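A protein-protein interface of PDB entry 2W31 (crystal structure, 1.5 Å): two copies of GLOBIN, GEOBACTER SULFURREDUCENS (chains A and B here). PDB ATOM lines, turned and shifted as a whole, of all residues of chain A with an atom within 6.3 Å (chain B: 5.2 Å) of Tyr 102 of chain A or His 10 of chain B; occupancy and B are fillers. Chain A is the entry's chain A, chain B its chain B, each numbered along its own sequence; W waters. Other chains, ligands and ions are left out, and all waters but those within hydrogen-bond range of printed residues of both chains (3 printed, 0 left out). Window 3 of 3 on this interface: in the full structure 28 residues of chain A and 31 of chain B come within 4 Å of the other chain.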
ATOM      1  N   TYR A  42     -22.613 -16.234  27.470  1.00  0.00           N
ATOM      2  CA  TYR A  42     -21.787 -15.174  26.905  1.00  0.00           C
ATOM      3  C   TYR A  42     -21.747 -13.952  27.857  1.00  0.00           C
ATOM      4  O   TYR A  42     -20.698 -13.343  28.059  1.00  0.00           O
ATOM      5  CB  TYR A  42     -22.395 -14.771  25.566  1.00  0.00           C
ATOM      6  CG  TYR A  42     -21.524 -13.958  24.633  1.00  0.00           C
ATOM      7  CD1 TYR A  42     -20.932 -14.540  23.504  1.00  0.00           C
ATOM      8  CD2 TYR A  42     -21.330 -12.590  24.842  1.00  0.00           C
ATOM      9  CE1 TYR A  42     -20.153 -13.763  22.599  1.00  0.00           C
ATOM     10  CE2 TYR A  42     -20.532 -11.806  23.935  1.00  0.00           C
ATOM     11  CZ  TYR A  42     -19.949 -12.413  22.841  1.00  0.00           C
ATOM     12  OH  TYR A  42     -19.218 -11.660  21.948  1.00  0.00           O
ATOM     13  N   LEU A  43     -22.899 -13.616  28.434  1.00  0.00           N
ATOM     14  CA  LEU A  43     -22.978 -12.481  29.360  1.00  0.00           C
ATOM     15  C   LEU A  43     -22.225 -12.730  30.666  1.00  0.00           C
ATOM     16  O   LEU A  43     -21.594 -11.803  31.222  1.00  0.00           O
ATOM     17  CB  LEU A  43     -24.438 -12.111  29.635  1.00  0.00           C
ATOM     18  CG  LEU A  43     -25.259 -11.602  28.430  1.00  0.00           C
ATOM     19  CD1 LEU A  43     -26.678 -11.223  28.872  1.00  0.00           C
ATOM     20  CD2 LEU A  43     -24.575 -10.442  27.731  1.00  0.00           C
ATOM     21  N   ILE A  46     -18.527 -11.794  30.578  1.00  0.00           N
ATOM     22  CA  ILE A  46     -18.079 -10.420  30.640  1.00  0.00           C
ATOM     23  C   ILE A  46     -18.391  -9.893  32.055  1.00  0.00           C
ATOM     24  O   ILE A  46     -19.557  -9.773  32.415  1.00  0.00           O
ATOM     25  CB  ILE A  46     -18.814  -9.495  29.596  1.00  0.00           C
ATOM     26  CG1 ILE A  46     -18.555  -9.943  28.148  1.00  0.00           C
ATOM     27  CG2 ILE A  46     -18.381  -8.047  29.769  1.00  0.00           C
ATOM     28  CD1 ILE A  46     -19.474  -9.300  27.116  1.00  0.00           C
ATOM     29  N   GLU A  48     -18.736  -6.974  33.516  1.00  0.00           N
ATOM     30  CA  GLU A  48     -19.743  -5.904  33.600  1.00  0.00           C
ATOM     31  C   GLU A  48     -21.239  -6.342  33.432  1.00  0.00           C
ATOM     32  O   GLU A  48     -22.147  -5.886  34.149  1.00  0.00           O
ATOM     33  CB  GLU A  48     -19.397  -4.800  32.621  1.00  0.00           C
ATOM     34  CG  GLU A  48     -18.092  -4.046  32.922  1.00  0.00           C
ATOM     35  CD  GLU A  48     -16.837  -4.684  32.300  1.00  0.00           C
ATOM     36  OE1 GLU A  48     -16.821  -5.901  31.977  1.00  0.00           O
ATOM     37  OE2 GLU A  48     -15.824  -3.953  32.147  1.00  0.00           O
ATOM     38  N   THR A  49     -21.505  -7.221  32.470  1.00  0.00           N
ATOM     39  CA  THR A  49     -22.847  -7.783  32.328  1.00  0.00           C
ATOM     40  C   THR A  49     -23.053  -8.901  33.373  1.00  0.00           C
ATOM     41  O   THR A  49     -24.171  -9.093  33.825  1.00  0.00           O
ATOM     42  CB  THR A  49     -23.095  -8.331  30.924  1.00  0.00           C
ATOM     43  OG1 THR A  49     -21.986  -9.158  30.519  1.00  0.00           O
ATOM     44  CG2 THR A  49     -23.247  -7.177  29.958  1.00  0.00           C
ATOM     45  N   PHE A  52     -25.102  -8.099  36.531  1.00  0.00           N
ATOM     46  CA  PHE A  52     -26.553  -8.016  36.517  1.00  0.00           C
ATOM     47  C   PHE A  52     -27.196  -9.349  36.681  1.00  0.00           C
ATOM     48  O   PHE A  52     -28.403  -9.410  36.868  1.00  0.00           O
ATOM     49  CB  PHE A  52     -27.078  -7.409  35.186  1.00  0.00           C
ATOM     50  CG  PHE A  52     -26.760  -5.959  35.030  1.00  0.00           C
ATOM     51  CD1 PHE A  52     -27.660  -4.982  35.496  1.00  0.00           C
ATOM     52  CD2 PHE A  52     -25.547  -5.557  34.490  1.00  0.00           C
ATOM     53  CE1 PHE A  52     -27.352  -3.627  35.378  1.00  0.00           C
ATOM     54  CE2 PHE A  52     -25.226  -4.181  34.365  1.00  0.00           C
ATOM     55  CZ  PHE A  52     -26.134  -3.224  34.836  1.00  0.00           C
ATOM     56  N   LEU A  98     -27.762  -0.527  32.786  1.00  0.00           N
ATOM     57  CA  LEU A  98     -26.981  -1.227  31.765  1.00  0.00           C
ATOM     58  C   LEU A  98     -26.524  -0.245  30.639  1.00  0.00           C
ATOM     59  O   LEU A  98     -27.343   0.476  30.040  1.00  0.00           O
ATOM     60  CB  LEU A  98     -27.825  -2.354  31.179  1.00  0.00           C
ATOM     61  CG  LEU A  98     -27.109  -3.238  30.150  1.00  0.00           C
ATOM     62  CD1 LEU A  98     -25.983  -4.048  30.791  1.00  0.00           C
ATOM     63  CD2 LEU A  98     -28.136  -4.130  29.429  1.00  0.00           C
ATOM     64  N   ASN A  99     -25.224  -0.213  30.357  1.00  0.00           N
ATOM     65  CA  ASN A  99     -24.743   0.650  29.266  1.00  0.00           C
ATOM     66  C   ASN A  99     -25.280   0.101  27.932  1.00  0.00           C
ATOM     67  O   ASN A  99     -25.250  -1.111  27.689  1.00  0.00           O
ATOM     68  CB  ASN A  99     -23.203   0.738  29.247  1.00  0.00           C
ATOM     69  CG  ASN A  99     -22.670   1.827  28.300  1.00  0.00           C
ATOM     70  OD1 ASN A  99     -22.754   1.724  27.077  1.00  0.00           O
ATOM     71  ND2 ASN A  99     -22.093   2.869  28.878  1.00  0.00           N
ATOM     72  N   ALA A 100     -25.738   1.005  27.066  1.00  0.00           N
ATOM     73  CA  ALA A 100     -26.302   0.627  25.747  1.00  0.00           C
ATOM     74  C   ALA A 100     -25.313  -0.239  24.940  1.00  0.00           C
ATOM     75  O   ALA A 100     -25.730  -1.089  24.122  1.00  0.00           O
ATOM     76  CB  ALA A 100     -26.642   1.873  24.940  1.00  0.00           C
ATOM     77  N   HIS A 101     -24.005  -0.007  25.081  1.00  0.00           N
ATOM     78  CA  HIS A 101     -22.986  -0.837  24.382  1.00  0.00           C
ATOM     79  C   HIS A 101     -23.275  -2.333  24.518  1.00  0.00           C
ATOM     80  O   HIS A 101     -23.089  -3.091  23.568  1.00  0.00           O
ATOM     81  CB  HIS A 101     -21.581  -0.507  24.925  1.00  0.00           C
ATOM     82  CG  HIS A 101     -20.522  -1.557  24.694  1.00  0.00           C
ATOM     83  ND1 HIS A 101     -20.056  -1.956  23.439  1.00  0.00           N
ATOM     84  CD2 HIS A 101     -19.808  -2.271  25.601  1.00  0.00           C
ATOM     85  CE1 HIS A 101     -19.102  -2.861  23.608  1.00  0.00           C
ATOM     86  NE2 HIS A 101     -18.955  -3.087  24.913  1.00  0.00           N
ATOM     87  N   TYR A 102     -23.729  -2.767  25.697  1.00  0.00           N
ATOM     88  CA  TYR A 102     -23.951  -4.207  25.925  1.00  0.00           C
ATOM     89  C   TYR A 102     -25.199  -4.717  25.215  1.00  0.00           C
ATOM     90  O   TYR A 102     -25.269  -5.911  24.889  1.00  0.00           O
ATOM     91  CB  TYR A 102     -23.963  -4.539  27.422  1.00  0.00           C
ATOM     92  CG  TYR A 102     -22.611  -4.228  28.028  1.00  0.00           C
ATOM     93  CD1 TYR A 102     -21.475  -5.000  27.695  1.00  0.00           C
ATOM     94  CD2 TYR A 102     -22.441  -3.119  28.871  1.00  0.00           C
ATOM     95  CE1 TYR A 102     -20.217  -4.704  28.210  1.00  0.00           C
ATOM     96  CE2 TYR A 102     -21.163  -2.800  29.395  1.00  0.00           C
ATOM     97  CZ  TYR A 102     -20.058  -3.599  29.051  1.00  0.00           C
ATOM     98  OH  TYR A 102     -18.776  -3.310  29.556  1.00  0.00           O
ATOM     99  N   VAL A 103     -26.147  -3.815  24.917  1.00  0.00           N
ATOM    100  CA  VAL A 103     -27.300  -4.170  24.073  1.00  0.00           C
ATOM    101  C   VAL A 103     -26.795  -4.472  22.649  1.00  0.00           C
ATOM    102  O   VAL A 103     -27.180  -5.488  22.031  1.00  0.00           O
ATOM    103  CB  VAL A 103     -28.441  -3.082  24.099  1.00  0.00           C
ATOM    104  CG1 VAL A 103     -29.569  -3.421  23.105  1.00  0.00           C
ATOM    105  CG2 VAL A 103     -29.039  -2.976  25.513  1.00  0.00           C
ATOM    106  N   ASN A 104     -25.939  -3.586  22.125  1.00  0.00           N
ATOM    107  CA  ASN A 104     -25.334  -3.891  20.814  1.00  0.00           C
ATOM    108  C   ASN A 104     -24.546  -5.208  20.829  1.00  0.00           C
ATOM    109  O   ASN A 104     -24.628  -6.025  19.868  1.00  0.00           O
ATOM    110  CB  ASN A 104     -24.445  -2.744  20.334  1.00  0.00           C
ATOM    111  CG  ASN A 104     -25.243  -1.463  19.982  1.00  0.00           C
ATOM    112  OD1 ASN A 104     -25.441  -1.094  18.777  1.00  0.00           O
ATOM    113  ND2 ASN A 104     -25.611  -0.730  21.008  1.00  0.00           N
ATOM    114  N   VAL A 105     -23.788  -5.424  21.900  1.00  0.00           N
ATOM    115  CA  VAL A 105     -23.012  -6.648  22.053  1.00  0.00           C
ATOM    116  C   VAL A 105     -23.914  -7.877  22.054  1.00  0.00           C
ATOM    117  O   VAL A 105     -23.650  -8.855  21.353  1.00  0.00           O
ATOM    118  CB  VAL A 105     -22.182  -6.632  23.350  1.00  0.00           C
ATOM    119  CG1 VAL A 105     -21.595  -8.008  23.622  1.00  0.00           C
ATOM    120  CG2 VAL A 105     -21.084  -5.583  23.264  1.00  0.00           C
ATOM    121  N   ALA A 106     -24.981  -7.822  22.844  1.00  0.00           N
ATOM    122  CA  ALA A 106     -25.903  -8.945  22.969  1.00  0.00           C
ATOM    123  C   ALA A 106     -26.579  -9.254  21.637  1.00  0.00           C
ATOM    124  O   ALA A 106     -26.852 -10.412  21.323  1.00  0.00           O
ATOM    125  CB  ALA A 106     -26.943  -8.661  24.041  1.00  0.00           C
ATOM    126  N   MET A 107     -26.845  -8.210  20.859  1.00  0.00           N
ATOM    127  CA  MET A 107     -27.584  -8.355  19.610  1.00  0.00           C
ATOM    128  C   MET A 107     -26.729  -9.018  18.536  1.00  0.00           C
ATOM    129  O   MET A 107     -27.246  -9.697  17.648  1.00  0.00           O
ATOM    130  CB  MET A 107     -28.081  -6.993  19.121  1.00  0.00           C
ATOM    131  CG  MET A 107     -29.081  -7.071  17.978  1.00  0.00           C
ATOM    132  SD  MET A 107     -30.570  -7.985  18.419  1.00  0.00           S
ATOM    133  CE  MET A 107     -31.516  -6.711  19.250  1.00  0.00           C
ATOM    134  N   VAL A 109     -24.596 -11.414  19.406  1.00  0.00           N
ATOM    135  CA  VAL A 109     -24.695 -12.818  19.791  1.00  0.00           C
ATOM    136  C   VAL A 109     -25.943 -13.479  19.142  1.00  0.00           C
ATOM    137  O   VAL A 109     -25.878 -14.575  18.583  1.00  0.00           O
ATOM    138  CB  VAL A 109     -24.752 -12.978  21.327  1.00  0.00           C
ATOM    139  CG1 VAL A 109     -24.907 -14.491  21.708  1.00  0.00           C
ATOM    140  CG2 VAL A 109     -23.512 -12.366  21.962  1.00  0.00           C
ATOM    141  N   LEU B   2     -14.568   3.022  25.558  1.00  0.00           N
ATOM    142  CA  LEU B   2     -13.706   1.845  25.731  1.00  0.00           C
ATOM    143  C   LEU B   2     -12.534   1.842  24.741  1.00  0.00           C
ATOM    144  O   LEU B   2     -12.577   2.494  23.690  1.00  0.00           O
ATOM    145  CB  LEU B   2     -14.505   0.525  25.589  1.00  0.00           C
ATOM    146  CG  LEU B   2     -15.568   0.258  26.675  1.00  0.00           C
ATOM    147  CD1 LEU B   2     -16.452  -0.916  26.304  1.00  0.00           C
ATOM    148  CD2 LEU B   2     -14.947   0.020  28.082  1.00  0.00           C
ATOM    149  N   GLU B   6     -10.732  -3.712  24.522  1.00  0.00           N
ATOM    150  CA  GLU B   6     -11.917  -4.080  25.330  1.00  0.00           C
ATOM    151  C   GLU B   6     -13.111  -4.378  24.438  1.00  0.00           C
ATOM    152  O   GLU B   6     -13.849  -5.359  24.667  1.00  0.00           O
ATOM    153  CB  GLU B   6     -12.267  -2.943  26.292  1.00  0.00           C
ATOM    154  CG  GLU B   6     -11.252  -2.820  27.414  1.00  0.00           C
ATOM    155  CD  GLU B   6     -11.507  -1.589  28.255  1.00  0.00           C
ATOM    156  OE1 GLU B   6     -11.251  -0.436  27.800  1.00  0.00           O
ATOM    157  OE2 GLU B   6     -12.003  -1.787  29.382  1.00  0.00           O
ATOM    158  N   ILE B   7     -13.286  -3.540  23.422  1.00  0.00           N
ATOM    159  CA  ILE B   7     -14.413  -3.749  22.444  1.00  0.00           C
ATOM    160  C   ILE B   7     -14.268  -5.075  21.717  1.00  0.00           C
ATOM    161  O   ILE B   7     -15.252  -5.812  21.534  1.00  0.00           O
ATOM    162  CB  ILE B   7     -14.541  -2.565  21.467  1.00  0.00           C
ATOM    163  CG1 ILE B   7     -14.929  -1.340  22.278  1.00  0.00           C
ATOM    164  CG2 ILE B   7     -15.543  -2.832  20.345  1.00  0.00           C
ATOM    165  CD1 ILE B   7     -14.654  -0.063  21.626  1.00  0.00           C
ATOM    166  N   LYS B   8     -13.046  -5.392  21.313  1.00  0.00           N
ATOM    167  CA  LYS B   8     -12.809  -6.661  20.626  1.00  0.00           C
ATOM    168  C   LYS B   8     -13.157  -7.797  21.578  1.00  0.00           C
ATOM    169  O   LYS B   8     -13.785  -8.773  21.148  1.00  0.00           O
ATOM    170  CB  LYS B   8     -11.364  -6.818  20.146  1.00  0.00           C
ATOM    171  CG  LYS B   8     -11.018  -5.990  18.972  1.00  0.00           C
ATOM    172  CD  LYS B   8      -9.540  -6.186  18.695  1.00  0.00           C
ATOM    173  CE  LYS B   8      -9.120  -5.559  17.407  1.00  0.00           C
ATOM    174  NZ  LYS B   8      -7.600  -5.580  17.221  1.00  0.00           N
ATOM    175  N   ALA B   9     -12.773  -7.690  22.863  1.00  0.00           N
ATOM    176  CA  ALA B   9     -13.023  -8.784  23.827  1.00  0.00           C
ATOM    177  C   ALA B   9     -14.535  -8.981  23.953  1.00  0.00           C
ATOM    178  O   ALA B   9     -15.024 -10.117  23.916  1.00  0.00           O
ATOM    179  CB  ALA B   9     -12.416  -8.484  25.164  1.00  0.00           C
ATOM    180  N   HIS B  10     -15.291  -7.886  24.034  1.00  0.00           N
ATOM    181  CA  HIS B  10     -16.753  -8.036  24.217  1.00  0.00           C
ATOM    182  C   HIS B  10     -17.419  -8.697  23.018  1.00  0.00           C
ATOM    183  O   HIS B  10     -18.348  -9.482  23.208  1.00  0.00           O
ATOM    184  CB  HIS B  10     -17.417  -6.710  24.528  1.00  0.00           C
ATOM    185  CG  HIS B  10     -16.917  -6.075  25.787  1.00  0.00           C
ATOM    186  ND1 HIS B  10     -17.164  -4.756  26.091  1.00  0.00           N
ATOM    187  CD2 HIS B  10     -16.143  -6.564  26.793  1.00  0.00           C
ATOM    188  CE1 HIS B  10     -16.610  -4.473  27.268  1.00  0.00           C
ATOM    189  NE2 HIS B  10     -15.965  -5.545  27.699  1.00  0.00           N
ATOM    190  N   TYR B  11     -16.957  -8.378  21.807  1.00  0.00           N
ATOM    191  CA  TYR B  11     -17.505  -8.991  20.581  1.00  0.00           C
ATOM    192  C   TYR B  11     -16.816 -10.299  20.190  1.00  0.00           C
ATOM    193  O   TYR B  11     -17.162 -10.894  19.162  1.00  0.00           O
ATOM    194  CB  TYR B  11     -17.413  -8.004  19.396  1.00  0.00           C
ATOM    195  CG  TYR B  11     -18.451  -6.900  19.433  1.00  0.00           C
ATOM    196  CD1 TYR B  11     -19.727  -7.109  18.891  1.00  0.00           C
ATOM    197  CD2 TYR B  11     -18.176  -5.636  20.016  1.00  0.00           C
ATOM    198  CE1 TYR B  11     -20.702  -6.108  18.910  1.00  0.00           C
ATOM    199  CE2 TYR B  11     -19.169  -4.615  20.087  1.00  0.00           C
ATOM    200  CZ  TYR B  11     -20.430  -4.861  19.519  1.00  0.00           C
ATOM    201  OH  TYR B  11     -21.406  -3.888  19.531  1.00  0.00           O
ATOM    202  N   ARG B  12     -15.871 -10.762  21.003  1.00  0.00           N
ATOM    203  CA  ARG B  12     -15.049 -11.954  20.662  1.00  0.00           C
ATOM    204  C   ARG B  12     -14.427 -11.836  19.258  1.00  0.00           C
ATOM    205  O   ARG B  12     -14.413 -12.795  18.447  1.00  0.00           O
ATOM    206  CB  ARG B  12     -15.823 -13.262  20.868  1.00  0.00           C
ATOM    207  CG  ARG B  12     -16.224 -13.474  22.283  1.00  0.00           C
ATOM    208  CD  ARG B  12     -16.767 -14.872  22.499  1.00  0.00           C
ATOM    209  NE  ARG B  12     -17.179 -15.024  23.890  1.00  0.00           N
ATOM    210  CZ  ARG B  12     -17.790 -16.102  24.379  1.00  0.00           C
ATOM    211  NH1 ARG B  12     -18.059 -17.129  23.593  1.00  0.00           N
ATOM    212  NH2 ARG B  12     -18.131 -16.145  25.662  1.00  0.00           N
HETATM  213  O   HOH W   1     -14.535  -6.262  29.981  1.00  0.00           O
HETATM  214  O   HOH W   2     -18.102 -13.588  26.944  1.00  0.00           O
HETATM  215  O   HOH W   3     -14.551  -2.945  29.495  1.00  0.00           O
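Printed residues of chain A within 4 Å of His 10 of chain B: Tyr 42, His 101, Tyr 102 and Val 105. Of the printed residues of chain A, Tyr 11 of chain B touches Tyr 42 (3.3 Å), His 101 (3.9 Å), Asn 104 (3.3 Å) and Val 105 (3.7 Å). Printed residues of chain B within 4 Å of Asn 104 of chain A: Tyr 11 (3.3 Å). Lys 8 of chain B touches none of the printed residues of chain A. Val 103 of chain A touches none of the printed residues of chain B. The nearest residue of chain B that does not touch Tyr 102 of chain A is Leu 2 of chain B (4.7 Å).
The backbone carbonyl oxygen of His 10 of chain B sits at hydrogen-bond distance from the side-chain hydroxyl of Tyr 42 of chain A (2.7 Å). A ring nitrogen (ND1) of His 10 of chain B sits at hydrogen-bond distance from a ring nitrogen (NE2) of His 101 of chain A, at 2.7 Å.
Among the printed residues, merely in contact across the chains: Tyr 42 of chain A with Tyr 11 of chain B, Tyr 42 of chain A with Arg 12 of chain B, His 101 of chain A with Leu 2 of chain B, His 101 of chain A with Tyr 11 of chain B, Tyr 102 of chain A with His 10 of chain B, Asn 104 of chain A with Tyr 11 of chain B, Val 105 of chain A with His 10 of chain B and Val 105 of chain A with Tyr 11 of chain B.
The side-chain amide nitrogen of Asn 104 of chain A sits at hydrogen-bond distance from the backbone carbonyl oxygen of Ala 100 of chain A (3.1 Å). OD1 of Asn 99 of chain A sits at hydrogen-bond distance from N of His 101 of chain A, at 2.9 Å.
Of the 8 printed residues of chain B, 4 touch a printed residue of chain A. Printed residues of chain A that touch a printed residue of chain B: Tyr 42, His 101, Tyr 102, Asn 104 and Val 105. Hydrophobic or aromatic side chains of chain A that line the printed part of chain B: Tyr 42, His 101, Tyr 102 and Val 105. Among the printed residues, 10 pairs touch across the chains.
Water W1 lies within hydrogen-bond range of NE2 of His 10 of chain B and OE1 of Glu 48 of chain A. Water W3 lies within hydrogen-bond range of the side-chain carboxylate of Glu 6 of chain B (2.8 Å), the side-chain carboxylate of Glu 48 of chain A (3.1 Å) and a ring nitrogen (NE2) of His 10 of chain B (3.5 Å). Water W2 bridges the backbone carbonyl oxygen (O) of Tyr 42 of chain A (2.8 Å) and the guanidinium group (NH2) of Arg 12 of chain B (2.9 Å).
No position is printed for both chains.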
